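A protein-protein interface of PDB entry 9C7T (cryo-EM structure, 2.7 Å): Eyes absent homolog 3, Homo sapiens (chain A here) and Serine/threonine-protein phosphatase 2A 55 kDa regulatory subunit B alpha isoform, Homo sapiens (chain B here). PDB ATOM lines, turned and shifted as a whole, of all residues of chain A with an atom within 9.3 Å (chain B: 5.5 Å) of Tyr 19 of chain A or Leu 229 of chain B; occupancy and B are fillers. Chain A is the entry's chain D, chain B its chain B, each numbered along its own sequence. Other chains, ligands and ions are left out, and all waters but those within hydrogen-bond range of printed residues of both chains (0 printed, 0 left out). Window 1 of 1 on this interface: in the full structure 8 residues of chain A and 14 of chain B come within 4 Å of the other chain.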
ATOM      1  N   TYR A  14     -17.359  -0.367  10.638  1.00  0.00           N
ATOM      2  CA  TYR A  14     -17.265   0.960  11.233  1.00  0.00           C
ATOM      3  C   TYR A  14     -15.825   1.472  11.229  1.00  0.00           C
ATOM      4  O   TYR A  14     -14.906   0.794  11.687  1.00  0.00           O
ATOM      5  CB  TYR A  14     -17.832   0.942  12.657  1.00  0.00           C
ATOM      6  CG  TYR A  14     -16.886   0.394  13.698  1.00  0.00           C
ATOM      7  CD1 TYR A  14     -16.602  -0.963  13.760  1.00  0.00           C
ATOM      8  CD2 TYR A  14     -16.270   1.232  14.615  1.00  0.00           C
ATOM      9  CE1 TYR A  14     -15.736  -1.470  14.708  1.00  0.00           C
ATOM     10  CE2 TYR A  14     -15.404   0.734  15.565  1.00  0.00           C
ATOM     11  CZ  TYR A  14     -15.141  -0.614  15.608  1.00  0.00           C
ATOM     12  OH  TYR A  14     -14.278  -1.102  16.558  1.00  0.00           O
ATOM     13  N   SER A  15     -15.630   2.664  10.662  1.00  0.00           N
ATOM     14  CA  SER A  15     -14.307   3.276  10.639  1.00  0.00           C
ATOM     15  C   SER A  15     -14.343   4.790  10.819  1.00  0.00           C
ATOM     16  O   SER A  15     -13.350   5.455  10.501  1.00  0.00           O
ATOM     17  CB  SER A  15     -13.580   2.931   9.333  1.00  0.00           C
ATOM     18  OG  SER A  15     -12.444   3.757   9.149  1.00  0.00           O
ATOM     19  N   ALA A  16     -15.447   5.363  11.306  1.00  0.00           N
ATOM     20  CA  ALA A  16     -15.602   6.810  11.329  1.00  0.00           C
ATOM     21  C   ALA A  16     -15.738   7.421  12.716  1.00  0.00           C
ATOM     22  O   ALA A  16     -14.996   8.360  13.023  1.00  0.00           O
ATOM     23  CB  ALA A  16     -16.822   7.230  10.495  1.00  0.00           C
ATOM     24  N   LYS A  17     -16.648   6.929  13.555  1.00  0.00           N
ATOM     25  CA  LYS A  17     -16.936   7.620  14.809  1.00  0.00           C
ATOM     26  C   LYS A  17     -15.798   7.456  15.817  1.00  0.00           C
ATOM     27  O   LYS A  17     -15.232   8.466  16.254  1.00  0.00           O
ATOM     28  CB  LYS A  17     -18.267   7.147  15.409  1.00  0.00           C
ATOM     29  CG  LYS A  17     -19.508   7.816  14.833  1.00  0.00           C
ATOM     30  CD  LYS A  17     -19.812   7.308  13.434  1.00  0.00           C
ATOM     31  CE  LYS A  17     -20.275   5.862  13.470  1.00  0.00           C
ATOM     32  NZ  LYS A  17     -20.639   5.357  12.119  1.00  0.00           N
ATOM     33  N   PRO A  18     -15.422   6.225  16.224  1.00  0.00           N
ATOM     34  CA  PRO A  18     -14.343   6.105  17.212  1.00  0.00           C
ATOM     35  C   PRO A  18     -12.963   6.229  16.587  1.00  0.00           C
ATOM     36  O   PRO A  18     -12.027   6.715  17.228  1.00  0.00           O
ATOM     37  CB  PRO A  18     -14.570   4.711  17.803  1.00  0.00           C
ATOM     38  CG  PRO A  18     -15.106   3.939  16.668  1.00  0.00           C
ATOM     39  CD  PRO A  18     -15.904   4.892  15.809  1.00  0.00           C
ATOM     40  N   TYR A  19     -12.828   5.779  15.338  1.00  0.00           N
ATOM     41  CA  TYR A  19     -11.553   5.814  14.633  1.00  0.00           C
ATOM     42  C   TYR A  19     -11.076   7.255  14.520  1.00  0.00           C
ATOM     43  O   TYR A  19     -10.078   7.636  15.140  1.00  0.00           O
ATOM     44  CB  TYR A  19     -11.691   5.199  13.239  1.00  0.00           C
ATOM     45  CG  TYR A  19     -11.702   3.685  13.194  1.00  0.00           C
ATOM     46  CD1 TYR A  19     -12.327   2.941  14.187  1.00  0.00           C
ATOM     47  CD2 TYR A  19     -11.109   3.000  12.141  1.00  0.00           C
ATOM     48  CE1 TYR A  19     -12.348   1.560  14.138  1.00  0.00           C
ATOM     49  CE2 TYR A  19     -11.126   1.619  12.084  1.00  0.00           C
ATOM     50  CZ  TYR A  19     -11.747   0.905  13.084  1.00  0.00           C
ATOM     51  OH  TYR A  19     -11.766  -0.468  13.032  1.00  0.00           O
ATOM     52  N   ALA A  20     -11.817   8.066  13.763  1.00  0.00           N
ATOM     53  CA  ALA A  20     -11.557   9.492  13.606  1.00  0.00           C
ATOM     54  C   ALA A  20     -10.081   9.810  13.406  1.00  0.00           C
ATOM     55  O   ALA A  20      -9.601   9.876  12.271  1.00  0.00           O
ATOM     56  CB  ALA A  20     -12.092  10.260  14.817  1.00  0.00           C
ATOM     57  N   HIS A  21      -9.363  10.014  14.512  1.00  0.00           N
ATOM     58  CA  HIS A  21      -8.007  10.547  14.482  1.00  0.00           C
ATOM     59  C   HIS A  21      -7.032   9.686  13.686  1.00  0.00           C
ATOM     60  O   HIS A  21      -6.054  10.210  13.145  1.00  0.00           O
ATOM     61  CB  HIS A  21      -7.488  10.742  15.910  1.00  0.00           C
ATOM     62  CG  HIS A  21      -7.479   9.491  16.732  1.00  0.00           C
ATOM     63  ND1 HIS A  21      -8.621   8.954  17.283  1.00  0.00           N
ATOM     64  CD2 HIS A  21      -6.462   8.680  17.109  1.00  0.00           C
ATOM     65  CE1 HIS A  21      -8.310   7.862  17.958  1.00  0.00           C
ATOM     66  NE2 HIS A  21      -7.006   7.674  17.869  1.00  0.00           N
ATOM     67  N   ILE A  22      -7.265   8.373  13.610  1.00  0.00           N
ATOM     68  CA  ILE A  22      -6.362   7.526  12.833  1.00  0.00           C
ATOM     69  C   ILE A  22      -6.433   7.894  11.357  1.00  0.00           C
ATOM     70  O   ILE A  22      -5.408   8.125  10.704  1.00  0.00           O
ATOM     71  CB  ILE A  22      -6.674   6.032  13.047  1.00  0.00           C
ATOM     72  CG1 ILE A  22      -6.442   5.609  14.495  1.00  0.00           C
ATOM     73  CG2 ILE A  22      -5.803   5.191  12.143  1.00  0.00           C
ATOM     74  CD1 ILE A  22      -7.662   5.687  15.358  1.00  0.00           C
ATOM     75  N   LEU A  23      -7.647   7.960  10.810  1.00  0.00           N
ATOM     76  CA  LEU A  23      -7.805   8.280   9.396  1.00  0.00           C
ATOM     77  C   LEU A  23      -7.619   9.764   9.120  1.00  0.00           C
ATOM     78  O   LEU A  23      -7.196  10.136   8.021  1.00  0.00           O
ATOM     79  CB  LEU A  23      -9.179   7.825   8.903  1.00  0.00           C
ATOM     80  CG  LEU A  23      -9.369   6.322   8.698  1.00  0.00           C
ATOM     81  CD1 LEU A  23      -9.861   5.667   9.977  1.00  0.00           C
ATOM     82  CD2 LEU A  23     -10.327   6.052   7.552  1.00  0.00           C
ATOM     83  N   SER A  24      -7.925  10.618  10.093  1.00  0.00           N
ATOM     84  CA  SER A  24      -7.838  12.057   9.888  1.00  0.00           C
ATOM     85  C   SER A  24      -6.380  12.497   9.882  1.00  0.00           C
ATOM     86  O   SER A  24      -5.660  12.301  10.867  1.00  0.00           O
ATOM     87  CB  SER A  24      -8.617  12.791  10.976  1.00  0.00           C
ATOM     88  OG  SER A  24      -9.983  12.418  10.961  1.00  0.00           O
ATOM     89  N   LEU B 202      -2.173   1.646  16.803  1.00  0.00           N
ATOM     90  CA  LEU B 202      -1.579   0.835  15.745  1.00  0.00           C
ATOM     91  C   LEU B 202      -0.188   0.302  16.045  1.00  0.00           C
ATOM     92  O   LEU B 202       0.303  -0.512  15.261  1.00  0.00           O
ATOM     93  CB  LEU B 202      -1.526   1.632  14.435  1.00  0.00           C
ATOM     94  CG  LEU B 202      -2.845   1.785  13.677  1.00  0.00           C
ATOM     95  CD1 LEU B 202      -2.729   2.863  12.622  1.00  0.00           C
ATOM     96  CD2 LEU B 202      -3.267   0.472  13.050  1.00  0.00           C
ATOM     97  N   PRO B 223      -1.197  -0.197   8.227  1.00  0.00           N
ATOM     98  CA  PRO B 223      -1.123  -0.553   6.809  1.00  0.00           C
ATOM     99  C   PRO B 223      -0.434   0.535   6.002  1.00  0.00           C
ATOM    100  O   PRO B 223      -0.385   1.704   6.391  1.00  0.00           O
ATOM    101  CB  PRO B 223      -2.591  -0.698   6.405  1.00  0.00           C
ATOM    102  CG  PRO B 223      -3.312   0.215   7.328  1.00  0.00           C
ATOM    103  CD  PRO B 223      -2.555   0.206   8.627  1.00  0.00           C
ATOM    104  N   ASN B 225      -1.415   1.663   3.040  1.00  0.00           N
ATOM    105  CA  ASN B 225      -2.478   2.552   2.585  1.00  0.00           C
ATOM    106  C   ASN B 225      -3.488   2.709   3.714  1.00  0.00           C
ATOM    107  O   ASN B 225      -4.148   1.741   4.105  1.00  0.00           O
ATOM    108  CB  ASN B 225      -3.139   2.001   1.325  1.00  0.00           C
ATOM    109  CG  ASN B 225      -3.919   3.057   0.569  1.00  0.00           C
ATOM    110  OD1 ASN B 225      -3.485   4.203   0.456  1.00  0.00           O
ATOM    111  ND2 ASN B 225      -5.077   2.675   0.045  1.00  0.00           N
ATOM    112  N   MET B 226      -3.620   3.928   4.230  1.00  0.00           N
ATOM    113  CA  MET B 226      -4.467   4.189   5.385  1.00  0.00           C
ATOM    114  C   MET B 226      -5.953   4.038   5.073  1.00  0.00           C
ATOM    115  O   MET B 226      -6.760   3.902   5.999  1.00  0.00           O
ATOM    116  CB  MET B 226      -4.172   5.587   5.937  1.00  0.00           C
ATOM    117  CG  MET B 226      -4.907   5.931   7.219  1.00  0.00           C
ATOM    118  SD  MET B 226      -4.426   4.860   8.587  1.00  0.00           S
ATOM    119  CE  MET B 226      -2.782   5.473   8.933  1.00  0.00           C
ATOM    120  N   GLU B 227      -6.335   4.024   3.799  1.00  0.00           N
ATOM    121  CA  GLU B 227      -7.711   3.751   3.411  1.00  0.00           C
ATOM    122  C   GLU B 227      -8.021   2.261   3.419  1.00  0.00           C
ATOM    123  O   GLU B 227      -9.166   1.873   3.167  1.00  0.00           O
ATOM    124  CB  GLU B 227      -8.007   4.341   2.032  1.00  0.00           C
ATOM    125  CG  GLU B 227      -7.994   5.862   1.981  1.00  0.00           C
ATOM    126  CD  GLU B 227      -6.600   6.437   1.837  1.00  0.00           C
ATOM    127  OE1 GLU B 227      -5.639   5.648   1.713  1.00  0.00           O
ATOM    128  OE2 GLU B 227      -6.463   7.677   1.849  1.00  0.00           O
ATOM    129  N   GLU B 228      -7.027   1.422   3.701  1.00  0.00           N
ATOM    130  CA  GLU B 228      -7.216  -0.016   3.842  1.00  0.00           C
ATOM    131  C   GLU B 228      -7.201  -0.424   5.310  1.00  0.00           C
ATOM    132  O   GLU B 228      -6.933  -1.579   5.640  1.00  0.00           O
ATOM    133  CB  GLU B 228      -6.149  -0.783   3.064  1.00  0.00           C
ATOM    134  CG  GLU B 228      -6.181  -0.552   1.566  1.00  0.00           C
ATOM    135  CD  GLU B 228      -4.916  -1.026   0.882  1.00  0.00           C
ATOM    136  OE1 GLU B 228      -3.994  -1.484   1.589  1.00  0.00           O
ATOM    137  OE2 GLU B 228      -4.841  -0.939  -0.362  1.00  0.00           O
ATOM    138  N   LEU B 229      -7.479   0.525   6.200  1.00  0.00           N
ATOM    139  CA  LEU B 229      -7.482   0.246   7.628  1.00  0.00           C
ATOM    140  C   LEU B 229      -8.665  -0.643   7.979  1.00  0.00           C
ATOM    141  O   LEU B 229      -9.798  -0.369   7.574  1.00  0.00           O
ATOM    142  CB  LEU B 229      -7.544   1.545   8.421  1.00  0.00           C
ATOM    143  CG  LEU B 229      -7.481   1.365   9.934  1.00  0.00           C
ATOM    144  CD1 LEU B 229      -6.122   0.835  10.341  1.00  0.00           C
ATOM    145  CD2 LEU B 229      -7.792   2.663  10.640  1.00  0.00           C
ATOM    146  N   THR B 230      -8.404  -1.709   8.734  1.00  0.00           N
ATOM    147  CA  THR B 230      -9.446  -2.630   9.151  1.00  0.00           C
ATOM    148  C   THR B 230      -9.388  -3.006  10.623  1.00  0.00           C
ATOM    149  O   THR B 230     -10.388  -3.505  11.149  1.00  0.00           O
ATOM    150  CB  THR B 230      -9.393  -3.915   8.312  1.00  0.00           C
ATOM    151  OG1 THR B 230     -10.512  -4.747   8.637  1.00  0.00           O
ATOM    152  CG2 THR B 230      -8.103  -4.674   8.578  1.00  0.00           C
ATOM    153  N   GLU B 231      -8.264  -2.783  11.298  1.00  0.00           N
ATOM    154  CA  GLU B 231      -8.110  -3.151  12.695  1.00  0.00           C
ATOM    155  C   GLU B 231      -7.325  -2.078  13.427  1.00  0.00           C
ATOM    156  O   GLU B 231      -6.500  -1.378  12.838  1.00  0.00           O
ATOM    157  CB  GLU B 231      -7.384  -4.486  12.859  1.00  0.00           C
ATOM    158  CG  GLU B 231      -8.265  -5.701  12.743  1.00  0.00           C
ATOM    159  CD  GLU B 231      -7.493  -6.983  12.948  1.00  0.00           C
ATOM    160  OE1 GLU B 231      -7.085  -7.252  14.096  1.00  0.00           O
ATOM    161  OE2 GLU B 231      -7.291  -7.722  11.963  1.00  0.00           O
ATOM    162  N   VAL B 232      -7.590  -1.964  14.727  1.00  0.00           N
ATOM    163  CA  VAL B 232      -6.802  -1.132  15.625  1.00  0.00           C
ATOM    164  C   VAL B 232      -6.542  -1.928  16.893  1.00  0.00           C
ATOM    165  O   VAL B 232      -7.267  -2.865  17.224  1.00  0.00           O
ATOM    166  CB  VAL B 232      -7.500   0.203  15.956  1.00  0.00           C
ATOM    167  CG1 VAL B 232      -7.515   1.106  14.743  1.00  0.00           C
ATOM    168  CG2 VAL B 232      -8.909  -0.050  16.442  1.00  0.00           C
ATOM    169  N   SER B 251      -9.934  -4.404  17.523  1.00  0.00           N
ATOM    170  CA  SER B 251     -11.327  -4.019  17.360  1.00  0.00           C
ATOM    171  C   SER B 251     -12.149  -5.075  16.641  1.00  0.00           C
ATOM    172  O   SER B 251     -13.370  -4.921  16.542  1.00  0.00           O
ATOM    173  CB  SER B 251     -11.419  -2.698  16.604  1.00  0.00           C
ATOM    174  OG  SER B 251     -10.723  -2.774  15.376  1.00  0.00           O
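The side-chain hydroxyl (OG) of Ser 251 of chain B lies within hydrogen-bond range of the side-chain hydroxyl (OH) of Tyr 19 of chain A (3.4 Å).
The backbone NH (N) of Ser 251 of chain B sits at hydrogen-bond distance from the backbone carbonyl oxygen (O) of Val 232 of chain B (3.1 Å).
The backbone carbonyl oxygen (O) of Tyr 19 of chain A is in hydrogen-bond range of a ring nitrogen (ND1) of His 21 of chain A, at 2.9 Å.
Among the printed residues, merely in contact across the chains: Tyr 14 of chain A with Ser 251 of chain B, Ile 22 of chain A with Leu 229 of chain B, Tyr 19 of chain A with Leu 229 of chain B, Leu 23 of chain A with Leu 229 of chain B, Ile 22 of chain A with Met 226 of chain B, Tyr 19 of chain A with Thr 230 of chain B and Ile 22 of chain A with Leu 202 of chain B.
Of the printed residues of chain B, Tyr 19 of chain A touches Leu 229, Thr 230 and Ser 251.
Printed residues of chain A within 4 Å of Leu 229 of chain B: Tyr 19 (3.7 Å), Ile 22 (3.6 Å) and Leu 23 (3.7 Å).
Printed residues of chain B within 4 Å of Ile 22 of chain A: Leu 202, Met 226 and Leu 229.
Printed residues of chain A within 4 Å of Met 226 of chain B: Ile 22 (3.8 Å).
Of the printed residues of chain B, Tyr 14 of chain A touches Ser 251 (3.3 Å).
Glu 231 of chain B touches none of the printed residues of chain A.
Glu 228 of chain B touches none of the printed residues of chain A.
The nearest residue of chain A that does not touch Leu 229 of chain B is Ser 15 of chain A (5.0 Å).
Of the 11 printed residues of chain A, 4 touch a printed residue of chain B.
Printed residues of chain A that touch a printed residue of chain B: Tyr 14, Tyr 19, Ile 22 and Leu 23.
Hydrophobic or aromatic side chains of chain A within 4 Å of the printed part of chain B: Tyr 14, Tyr 19, Ile 22 and Leu 23.
Hydrophobic or aromatic side chains of chain B that line the printed part of chain A: Leu 202, Met 226 and Leu 229.
Along chain B the printed residues that touch a printed residue of chain A span positions 202 to 251.
Among the printed residues, no Asp or Glu carboxylate lies within 4 Å of a Lys or Arg side-chain nitrogen of the other chain.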
